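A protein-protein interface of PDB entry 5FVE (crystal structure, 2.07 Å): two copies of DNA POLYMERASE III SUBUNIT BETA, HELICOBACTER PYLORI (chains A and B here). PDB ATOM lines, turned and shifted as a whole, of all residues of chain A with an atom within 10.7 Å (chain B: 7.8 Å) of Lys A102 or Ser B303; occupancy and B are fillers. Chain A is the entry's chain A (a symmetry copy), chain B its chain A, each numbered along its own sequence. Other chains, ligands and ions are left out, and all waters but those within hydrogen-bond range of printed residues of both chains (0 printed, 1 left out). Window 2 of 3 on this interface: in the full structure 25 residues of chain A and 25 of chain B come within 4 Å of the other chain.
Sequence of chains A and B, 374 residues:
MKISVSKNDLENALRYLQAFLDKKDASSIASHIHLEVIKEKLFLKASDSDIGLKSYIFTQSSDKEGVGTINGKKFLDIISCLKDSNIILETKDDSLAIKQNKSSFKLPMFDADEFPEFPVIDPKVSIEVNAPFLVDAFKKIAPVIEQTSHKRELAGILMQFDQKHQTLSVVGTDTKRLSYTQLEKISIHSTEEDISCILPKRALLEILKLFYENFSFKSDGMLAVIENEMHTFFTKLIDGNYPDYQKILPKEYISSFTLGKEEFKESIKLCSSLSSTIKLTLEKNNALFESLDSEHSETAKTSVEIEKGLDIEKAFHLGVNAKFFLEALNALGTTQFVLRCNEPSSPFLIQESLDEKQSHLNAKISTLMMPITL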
ATOM      1  N   CYS A  81      25.213 -13.729  29.672  1.00  0.00           N
ATOM      2  CA  CYS A  81      25.366 -13.374  28.256  1.00  0.00           C
ATOM      3  C   CYS A  81      24.492 -14.223  27.301  1.00  0.00           C
ATOM      4  O   CYS A  81      24.572 -14.065  26.081  1.00  0.00           O
ATOM      5  CB  CYS A  81      26.859 -13.436  27.852  1.00  0.00           C
ATOM      6  SG  CYS A  81      27.787 -11.943  28.305  1.00  0.00           S
ATOM      7  N   LEU A  82      23.655 -15.101  27.850  1.00  0.00           N
ATOM      8  CA  LEU A  82      22.754 -15.930  27.051  1.00  0.00           C
ATOM      9  C   LEU A  82      21.352 -15.335  26.938  1.00  0.00           C
ATOM     10  O   LEU A  82      20.973 -14.418  27.672  1.00  0.00           O
ATOM     11  CB  LEU A  82      22.672 -17.348  27.632  1.00  0.00           C
ATOM     12  CG  LEU A  82      23.986 -18.131  27.553  1.00  0.00           C
ATOM     13  CD1 LEU A  82      23.847 -19.508  28.193  1.00  0.00           C
ATOM     14  CD2 LEU A  82      24.461 -18.255  26.118  1.00  0.00           C
ATOM     15  N   LYS A  83      20.594 -15.891  25.998  1.00  0.00           N
ATOM     16  CA  LYS A  83      19.208 -15.488  25.744  1.00  0.00           C
ATOM     17  C   LYS A  83      18.282 -16.256  26.670  1.00  0.00           C
ATOM     18  O   LYS A  83      18.724 -17.154  27.378  1.00  0.00           O
ATOM     19  CB  LYS A  83      18.873 -15.721  24.274  1.00  0.00           C
ATOM     20  CG  LYS A  83      19.679 -14.804  23.363  1.00  0.00           C
ATOM     21  CD  LYS A  83      19.798 -15.313  21.942  1.00  0.00           C
ATOM     22  CE  LYS A  83      20.477 -14.262  21.078  1.00  0.00           C
ATOM     23  NZ  LYS A  83      20.653 -14.717  19.675  1.00  0.00           N
ATOM     24  N   SER A  85      15.925 -18.516  26.247  1.00  0.00           N
ATOM     25  CA  SER A  85      15.638 -19.935  25.995  1.00  0.00           C
ATOM     26  C   SER A  85      16.363 -20.864  26.981  1.00  0.00           C
ATOM     27  O   SER A  85      17.427 -20.513  27.513  1.00  0.00           O
ATOM     28  CB  SER A  85      16.029 -20.302  24.567  1.00  0.00           C
ATOM     29  OG  SER A  85      17.409 -20.062  24.347  1.00  0.00           O
ATOM     30  N   ASN A  86      15.789 -22.045  27.207  1.00  0.00           N
ATOM     31  CA  ASN A  86      16.359 -23.030  28.135  1.00  0.00           C
ATOM     32  C   ASN A  86      17.829 -23.353  27.862  1.00  0.00           C
ATOM     33  O   ASN A  86      18.298 -23.257  26.728  1.00  0.00           O
ATOM     34  CB  ASN A  86      15.551 -24.340  28.115  1.00  0.00           C
ATOM     35  CG  ASN A  86      14.212 -24.225  28.837  1.00  0.00           C
ATOM     36  OD1 ASN A  86      13.948 -23.258  29.551  1.00  0.00           O
ATOM     37  ND2 ASN A  86      13.360 -25.231  28.655  1.00  0.00           N
ATOM     38  N   ILE A  87      18.530 -23.744  28.925  1.00  0.00           N
ATOM     39  CA  ILE A  87      19.962 -24.053  28.889  1.00  0.00           C
ATOM     40  C   ILE A  87      20.188 -25.507  29.286  1.00  0.00           C
ATOM     41  O   ILE A  87      19.681 -25.964  30.314  1.00  0.00           O
ATOM     42  CB  ILE A  87      20.730 -23.173  29.887  1.00  0.00           C
ATOM     43  CG1 ILE A  87      20.567 -21.702  29.509  1.00  0.00           C
ATOM     44  CG2 ILE A  87      22.212 -23.558  29.951  1.00  0.00           C
ATOM     45  CD1 ILE A  87      20.893 -20.768  30.642  1.00  0.00           C
ATOM     46  N   ILE A  88      20.988 -26.201  28.491  1.00  0.00           N
ATOM     47  CA  ILE A  88      21.351 -27.585  28.744  1.00  0.00           C
ATOM     48  C   ILE A  88      22.672 -27.602  29.513  1.00  0.00           C
ATOM     49  O   ILE A  88      23.669 -27.036  29.046  1.00  0.00           O
ATOM     50  CB  ILE A  88      21.495 -28.355  27.416  1.00  0.00           C
ATOM     51  CG1 ILE A  88      20.120 -28.462  26.735  1.00  0.00           C
ATOM     52  CG2 ILE A  88      22.108 -29.736  27.635  1.00  0.00           C
ATOM     53  CD1 ILE A  88      20.178 -28.879  25.278  1.00  0.00           C
ATOM     54  N   ILE A  98      27.768 -26.436  28.766  1.00  0.00           N
ATOM     55  CA  ILE A  98      26.635 -25.517  28.867  1.00  0.00           C
ATOM     56  C   ILE A  98      26.269 -25.192  27.427  1.00  0.00           C
ATOM     57  O   ILE A  98      27.142 -24.780  26.658  1.00  0.00           O
ATOM     58  CB  ILE A  98      27.013 -24.226  29.616  1.00  0.00           C
ATOM     59  CG1 ILE A  98      27.546 -24.552  31.017  1.00  0.00           C
ATOM     60  CG2 ILE A  98      25.812 -23.277  29.722  1.00  0.00           C
ATOM     61  CD1 ILE A  98      28.210 -23.388  31.727  1.00  0.00           C
ATOM     62  N   LYS A  99      25.013 -25.409  27.048  1.00  0.00           N
ATOM     63  CA  LYS A  99      24.587 -25.236  25.657  1.00  0.00           C
ATOM     64  C   LYS A  99      23.248 -24.532  25.558  1.00  0.00           C
ATOM     65  O   LYS A  99      22.323 -24.776  26.356  1.00  0.00           O
ATOM     66  CB  LYS A  99      24.504 -26.574  24.930  1.00  0.00           C
ATOM     67  CG  LYS A  99      25.727 -27.441  25.154  1.00  0.00           C
ATOM     68  CD  LYS A  99      26.003 -28.415  24.029  1.00  0.00           C
ATOM     69  CE  LYS A  99      27.397 -28.990  24.198  1.00  0.00           C
ATOM     70  NZ  LYS A  99      27.786 -29.819  23.032  1.00  0.00           N
ATOM     71  N   GLN A 100      23.165 -23.661  24.557  1.00  0.00           N
ATOM     72  CA  GLN A 100      21.939 -22.976  24.191  1.00  0.00           C
ATOM     73  C   GLN A 100      22.041 -22.631  22.706  1.00  0.00           C
ATOM     74  O   GLN A 100      22.856 -21.777  22.317  1.00  0.00           O
ATOM     75  CB  GLN A 100      21.774 -21.717  25.036  1.00  0.00           C
ATOM     76  CG  GLN A 100      20.382 -21.109  24.967  1.00  0.00           C
ATOM     77  CD  GLN A 100      20.367 -19.656  25.381  1.00  0.00           C
ATOM     78  OE1 GLN A 100      20.944 -18.804  24.698  1.00  0.00           O
ATOM     79  NE2 GLN A 100      19.710 -19.363  26.489  1.00  0.00           N
ATOM     80  N   ASN A 101      21.252 -23.331  21.883  1.00  0.00           N
ATOM     81  CA  ASN A 101      21.189 -23.092  20.437  1.00  0.00           C
ATOM     82  C   ASN A 101      22.588 -23.238  19.808  1.00  0.00           C
ATOM     83  O   ASN A 101      23.173 -24.314  19.885  1.00  0.00           O
ATOM     84  CB  ASN A 101      20.536 -21.721  20.138  1.00  0.00           C
ATOM     85  CG  ASN A 101      19.134 -21.587  20.712  1.00  0.00           C
ATOM     86  OD1 ASN A 101      18.757 -20.523  21.220  1.00  0.00           O
ATOM     87  ND2 ASN A 101      18.346 -22.657  20.621  1.00  0.00           N
ATOM     88  N   LYS A 102      23.144 -22.162  19.244  1.00  0.00           N
ATOM     89  CA  LYS A 102      24.454 -22.210  18.597  1.00  0.00           C
ATOM     90  C   LYS A 102      25.627 -21.986  19.563  1.00  0.00           C
ATOM     91  O   LYS A 102      26.777 -22.160  19.170  1.00  0.00           O
ATOM     92  CB  LYS A 102      24.508 -21.169  17.470  1.00  0.00           C
ATOM     93  CG  LYS A 102      23.508 -21.417  16.340  1.00  0.00           C
ATOM     94  CD  LYS A 102      23.154 -20.126  15.611  1.00  0.00           C
ATOM     95  CE  LYS A 102      22.073 -20.334  14.560  1.00  0.00           C
ATOM     96  NZ  LYS A 102      22.591 -21.045  13.366  1.00  0.00           N
ATOM     97  N   SER A 103      25.342 -21.604  20.807  1.00  0.00           N
ATOM     98  CA  SER A 103      26.380 -21.265  21.792  1.00  0.00           C
ATOM     99  C   SER A 103      26.672 -22.431  22.738  1.00  0.00           C
ATOM    100  O   SER A 103      25.742 -22.995  23.323  1.00  0.00           O
ATOM    101  CB  SER A 103      25.939 -20.066  22.628  1.00  0.00           C
ATOM    102  OG  SER A 103      25.683 -18.927  21.827  1.00  0.00           O
ATOM    103  N   SER A 104      27.948 -22.778  22.900  1.00  0.00           N
ATOM    104  CA  SER A 104      28.345 -23.849  23.833  1.00  0.00           C
ATOM    105  C   SER A 104      29.621 -23.514  24.608  1.00  0.00           C
ATOM    106  O   SER A 104      30.510 -22.851  24.088  1.00  0.00           O
ATOM    107  CB  SER A 104      28.483 -25.191  23.103  1.00  0.00           C
ATOM    108  OG  SER A 104      29.576 -25.187  22.211  1.00  0.00           O
ATOM    109  N   PHE A 105      29.675 -23.955  25.865  1.00  0.00           N
ATOM    110  CA  PHE A 105      30.775 -23.654  26.788  1.00  0.00           C
ATOM    111  C   PHE A 105      31.211 -24.906  27.536  1.00  0.00           C
ATOM    112  O   PHE A 105      30.388 -25.784  27.795  1.00  0.00           O
ATOM    113  CB  PHE A 105      30.356 -22.639  27.841  1.00  0.00           C
ATOM    114  CG  PHE A 105      29.673 -21.421  27.291  1.00  0.00           C
ATOM    115  CD1 PHE A 105      28.347 -21.482  26.886  1.00  0.00           C
ATOM    116  CD2 PHE A 105      30.343 -20.207  27.212  1.00  0.00           C
ATOM    117  CE1 PHE A 105      27.706 -20.365  26.382  1.00  0.00           C
ATOM    118  CE2 PHE A 105      29.707 -19.080  26.719  1.00  0.00           C
ATOM    119  CZ  PHE A 105      28.384 -19.159  26.301  1.00  0.00           C
ATOM    120  N   GLU B 263      24.636  -8.626  16.203  1.00  0.00           N
ATOM    121  CA  GLU B 263      25.003 -10.041  16.313  1.00  0.00           C
ATOM    122  C   GLU B 263      26.476 -10.231  16.643  1.00  0.00           C
ATOM    123  O   GLU B 263      26.803 -11.088  17.460  1.00  0.00           O
ATOM    124  CB  GLU B 263      24.609 -10.836  15.055  1.00  0.00           C
ATOM    125  CG  GLU B 263      23.110 -11.067  15.004  1.00  0.00           C
ATOM    126  CD  GLU B 263      22.668 -12.082  13.957  1.00  0.00           C
ATOM    127  OE1 GLU B 263      23.451 -12.463  13.063  1.00  0.00           O
ATOM    128  OE2 GLU B 263      21.499 -12.479  14.039  1.00  0.00           O
ATOM    129  N   SER B 267      27.906 -11.794  20.164  1.00  0.00           N
ATOM    130  CA  SER B 267      28.755 -12.965  20.048  1.00  0.00           C
ATOM    131  C   SER B 267      30.103 -12.728  20.717  1.00  0.00           C
ATOM    132  O   SER B 267      30.667 -13.627  21.346  1.00  0.00           O
ATOM    133  CB  SER B 267      28.937 -13.355  18.580  1.00  0.00           C
ATOM    134  OG  SER B 267      27.668 -13.599  17.990  1.00  0.00           O
ATOM    135  N   LEU B 270      29.700 -12.491  24.538  1.00  0.00           N
ATOM    136  CA  LEU B 270      29.510 -13.854  24.979  1.00  0.00           C
ATOM    137  C   LEU B 270      30.842 -14.578  25.135  1.00  0.00           C
ATOM    138  O   LEU B 270      31.105 -15.119  26.212  1.00  0.00           O
ATOM    139  CB  LEU B 270      28.553 -14.586  24.034  1.00  0.00           C
ATOM    140  CG  LEU B 270      28.182 -16.022  24.365  1.00  0.00           C
ATOM    141  CD1 LEU B 270      26.736 -16.325  24.006  1.00  0.00           C
ATOM    142  CD2 LEU B 270      29.108 -16.999  23.665  1.00  0.00           C
ATOM    143  N   CYS B 271      31.696 -14.560  24.102  1.00  0.00           N
ATOM    144  CA  CYS B 271      32.979 -15.280  24.177  1.00  0.00           C
ATOM    145  C   CYS B 271      33.949 -14.611  25.140  1.00  0.00           C
ATOM    146  O   CYS B 271      34.779 -15.283  25.742  1.00  0.00           O
ATOM    147  CB  CYS B 271      33.614 -15.466  22.798  1.00  0.00           C
ATOM    148  SG  CYS B 271      32.626 -16.545  21.752  1.00  0.00           S
ATOM    149  N   THR B 281      36.052 -16.838  12.828  1.00  0.00           N
ATOM    150  CA  THR B 281      36.118 -17.579  11.565  1.00  0.00           C
ATOM    151  C   THR B 281      34.941 -17.169  10.696  1.00  0.00           C
ATOM    152  O   THR B 281      33.787 -17.320  11.093  1.00  0.00           O
ATOM    153  CB  THR B 281      36.040 -19.101  11.777  1.00  0.00           C
ATOM    154  OG1 THR B 281      37.049 -19.524  12.708  1.00  0.00           O
ATOM    155  CG2 THR B 281      36.192 -19.856  10.446  1.00  0.00           C
ATOM    156  N   ASN B 285      28.334 -18.564   4.643  1.00  0.00           N
ATOM    157  CA  ASN B 285      27.041 -18.308   5.296  1.00  0.00           C
ATOM    158  C   ASN B 285      27.089 -18.378   6.818  1.00  0.00           C
ATOM    159  O   ASN B 285      26.063 -18.590   7.464  1.00  0.00           O
ATOM    160  CB  ASN B 285      25.976 -19.260   4.735  1.00  0.00           C
ATOM    161  CG  ASN B 285      25.671 -18.975   3.275  1.00  0.00           C
ATOM    162  OD1 ASN B 285      26.085 -19.729   2.391  1.00  0.00           O
ATOM    163  ND2 ASN B 285      24.977 -17.859   3.011  1.00  0.00           N
ATOM    164  N   ASN B 286      28.266 -18.143   7.391  1.00  0.00           N
ATOM    165  CA  ASN B 286      28.458 -18.329   8.825  1.00  0.00           C
ATOM    166  C   ASN B 286      29.610 -17.532   9.414  1.00  0.00           C
ATOM    167  O   ASN B 286      30.659 -17.383   8.784  1.00  0.00           O
ATOM    168  CB  ASN B 286      28.723 -19.806   9.091  1.00  0.00           C
ATOM    169  CG  ASN B 286      27.772 -20.385  10.087  1.00  0.00           C
ATOM    170  OD1 ASN B 286      28.115 -20.551  11.255  1.00  0.00           O
ATOM    171  ND2 ASN B 286      26.554 -20.675   9.645  1.00  0.00           N
ATOM    172  N   ALA B 287      29.420 -17.038  10.633  1.00  0.00           N
ATOM    173  CA  ALA B 287      30.502 -16.454  11.410  1.00  0.00           C
ATOM    174  C   ALA B 287      30.617 -17.241  12.692  1.00  0.00           C
ATOM    175  O   ALA B 287      29.624 -17.368  13.391  1.00  0.00           O
ATOM    176  CB  ALA B 287      30.217 -14.992  11.702  1.00  0.00           C
ATOM    177  N   LEU B 288      31.801 -17.791  12.983  1.00  0.00           N
ATOM    178  CA  LEU B 288      32.052 -18.546  14.231  1.00  0.00           C
ATOM    179  C   LEU B 288      32.956 -17.737  15.132  1.00  0.00           C
ATOM    180  O   LEU B 288      33.891 -17.097  14.656  1.00  0.00           O
ATOM    181  CB  LEU B 288      32.741 -19.899  13.968  1.00  0.00           C
ATOM    182  CG  LEU B 288      32.297 -20.717  12.763  1.00  0.00           C
ATOM    183  CD1 LEU B 288      33.115 -22.005  12.655  1.00  0.00           C
ATOM    184  CD2 LEU B 288      30.814 -21.042  12.846  1.00  0.00           C
ATOM    185  N   PHE B 289      32.680 -17.793  16.427  1.00  0.00           N
ATOM    186  CA  PHE B 289      33.437 -17.074  17.441  1.00  0.00           C
ATOM    187  C   PHE B 289      33.869 -18.081  18.482  1.00  0.00           C
ATOM    188  O   PHE B 289      33.057 -18.891  18.910  1.00  0.00           O
ATOM    189  CB  PHE B 289      32.555 -16.045  18.134  1.00  0.00           C
ATOM    190  CG  PHE B 289      31.924 -15.042  17.205  1.00  0.00           C
ATOM    191  CD1 PHE B 289      30.802 -15.383  16.442  1.00  0.00           C
ATOM    192  CD2 PHE B 289      32.416 -13.747  17.129  1.00  0.00           C
ATOM    193  CE1 PHE B 289      30.207 -14.445  15.609  1.00  0.00           C
ATOM    194  CE2 PHE B 289      31.828 -12.810  16.295  1.00  0.00           C
ATOM    195  CZ  PHE B 289      30.724 -13.163  15.538  1.00  0.00           C
ATOM    196  N   GLU B 290      35.137 -18.035  18.878  1.00  0.00           N
ATOM    197  CA  GLU B 290      35.664 -18.923  19.913  1.00  0.00           C
ATOM    198  C   GLU B 290      36.634 -18.164  20.789  1.00  0.00           C
ATOM    199  O   GLU B 290      37.478 -17.439  20.267  1.00  0.00           O
ATOM    200  CB  GLU B 290      36.419 -20.107  19.305  1.00  0.00           C
ATOM    201  CG  GLU B 290      35.675 -20.856  18.215  1.00  0.00           C
ATOM    202  CD  GLU B 290      36.482 -22.019  17.669  1.00  0.00           C
ATOM    203  OE1 GLU B 290      36.699 -22.992  18.419  1.00  0.00           O
ATOM    204  OE2 GLU B 290      36.897 -21.947  16.495  1.00  0.00           O
ATOM    205  N   LYS B 301      32.107 -20.771  22.802  1.00  0.00           N
ATOM    206  CA  LYS B 301      31.901 -20.772  21.356  1.00  0.00           C
ATOM    207  C   LYS B 301      30.486 -20.343  21.010  1.00  0.00           C
ATOM    208  O   LYS B 301      29.519 -20.652  21.737  1.00  0.00           O
ATOM    209  CB  LYS B 301      32.089 -22.159  20.764  1.00  0.00           C
ATOM    210  CG  LYS B 301      33.485 -22.739  20.872  1.00  0.00           C
ATOM    211  CD  LYS B 301      33.522 -24.207  20.449  1.00  0.00           C
ATOM    212  CE  LYS B 301      32.958 -24.439  19.049  1.00  0.00           C
ATOM    213  NZ  LYS B 301      33.227 -25.821  18.557  1.00  0.00           N
ATOM    214  N   THR B 302      30.363 -19.647  19.885  1.00  0.00           N
ATOM    215  CA  THR B 302      29.058 -19.429  19.294  1.00  0.00           C
ATOM    216  C   THR B 302      29.184 -19.157  17.819  1.00  0.00           C
ATOM    217  O   THR B 302      30.295 -19.025  17.305  1.00  0.00           O
ATOM    218  CB  THR B 302      28.264 -18.318  20.009  1.00  0.00           C
ATOM    219  OG1 THR B 302      26.879 -18.425  19.638  1.00  0.00           O
ATOM    220  CG2 THR B 302      28.811 -16.930  19.690  1.00  0.00           C
ATOM    221  N   SER B 303      28.048 -19.091  17.142  1.00  0.00           N
ATOM    222  CA  SER B 303      28.037 -18.699  15.736  1.00  0.00           C
ATOM    223  C   SER B 303      26.743 -18.030  15.346  1.00  0.00           C
ATOM    224  O   SER B 303      25.730 -18.198  16.013  1.00  0.00           O
ATOM    225  CB  SER B 303      28.265 -19.918  14.856  1.00  0.00           C
ATOM    226  OG  SER B 303      27.167 -20.793  14.940  1.00  0.00           O
ATOM    227  N   VAL B 304      26.789 -17.273  14.251  1.00  0.00           N
ATOM    228  CA  VAL B 304      25.592 -16.686  13.657  1.00  0.00           C
ATOM    229  C   VAL B 304      25.541 -16.988  12.164  1.00  0.00           C
ATOM    230  O   VAL B 304      26.574 -17.100  11.500  1.00  0.00           O
ATOM    231  CB  VAL B 304      25.485 -15.150  13.898  1.00  0.00           C
ATOM    232  CG1 VAL B 304      25.455 -14.853  15.402  1.00  0.00           C
ATOM    233  CG2 VAL B 304      26.592 -14.379  13.209  1.00  0.00           C
ATOM    234  N   GLU B 305      24.326 -17.112  11.657  1.00  0.00           N
ATOM    235  CA  GLU B 305      24.113 -17.326  10.244  1.00  0.00           C
ATOM    236  C   GLU B 305      24.256 -15.998   9.490  1.00  0.00           C
ATOM    237  O   GLU B 305      23.725 -14.976   9.927  1.00  0.00           O
ATOM    238  CB  GLU B 305      22.728 -17.908  10.025  1.00  0.00           C
ATOM    239  CG  GLU B 305      22.516 -18.429   8.622  1.00  0.00           C
ATOM    240  CD  GLU B 305      21.132 -19.001   8.430  1.00  0.00           C
ATOM    241  OE1 GLU B 305      20.498 -19.385   9.440  1.00  0.00           O
ATOM    242  OE2 GLU B 305      20.683 -19.035   7.267  1.00  0.00           O
ATOM    243  N   ILE B 306      24.991 -16.031   8.378  1.00  0.00           N
ATOM    244  CA  ILE B 306      25.069 -14.934   7.414  1.00  0.00           C
ATOM    245  C   ILE B 306      24.229 -15.292   6.173  1.00  0.00           C
ATOM    246  O   ILE B 306      24.654 -16.101   5.343  1.00  0.00           O
ATOM    247  CB  ILE B 306      26.527 -14.646   7.015  1.00  0.00           C
ATOM    248  CG1 ILE B 306      27.381 -14.409   8.268  1.00  0.00           C
ATOM    249  CG2 ILE B 306      26.596 -13.414   6.126  1.00  0.00           C
ATOM    250  CD1 ILE B 306      28.861 -14.293   8.006  1.00  0.00           C
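The side-chain hydroxyl of Ser A103 is in hydrogen-bond range of the side-chain hydroxyl of Thr B302 (2.5 Å).
O of Lys B301 lies within hydrogen-bond range of N of Ser A104 (2.9 Å).
No position is printed for both chains.
O of Ile A98 is in hydrogen-bond range of N of Phe A105 (2.8 Å).
O of Thr B302 lies within hydrogen-bond range of N of Phe B289 (2.8 Å).
Printed residues of chain B that touch a printed residue of chain A: Leu B270, Lys B301, Thr B302 and Ser B303.
Printed residues of chain A that touch a printed residue of chain B: Cys A81, Leu A82, Lys A102, Ser A103, Ser A104 and Phe A105.
Hydrophobic or aromatic side chains of chain A within 4 Å of the printed part of chain B: Leu A82 and Phe A105.
Among the printed residues, 9 pairs touch across the chains.
Among the printed residues, no Asp or Glu carboxylate lies within 4 Å of a Lys or Arg side-chain nitrogen of the other chain.
Among the printed residues, pairs that only touch across the chains: Ser A103 with Lys B301 (3.2 Å), Lys A102 with Ser B303 (3.2 Å), Phe A105 with Leu B270 (3.5 Å), Ser A103 with Leu B270 (3.6 Å), Lys A102 with Thr B302 (3.6 Å), Leu A82 with Leu B270 (3.7 Å) and Cys A81 with Leu B270 (3.8 Å).
Of chain B, only Thr B302 and Ser B303 come within 4 Å of Lys A102.
Ser B303 touches just one residue of chain A: Lys A102 (3.2 Å).
No residue of chain A comes within 4 Å of Ala B287.
No residue of chain A comes within 4 Å of Val B304.
Of the printed residues of chain A, Lys B301 touches Ser A103 (3.2 Å) and Ser A104 (2.9 Å).
Of the printed residues of chain B, Ser A104 touches Lys B301 (2.9 Å).
Of the printed residues of chain B, Phe A105 touches Leu B270 (3.5 Å).
Printed residues of chain B within 4 Å of Leu A82: Leu B270.
Printed residues of chain A within 4 Å of Leu B270: Cys A81, Leu A82, Ser A103 and Phe A105.
The nearest residue of chain B that does not touch Lys A102 is Lys B301 (4.05 Å).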
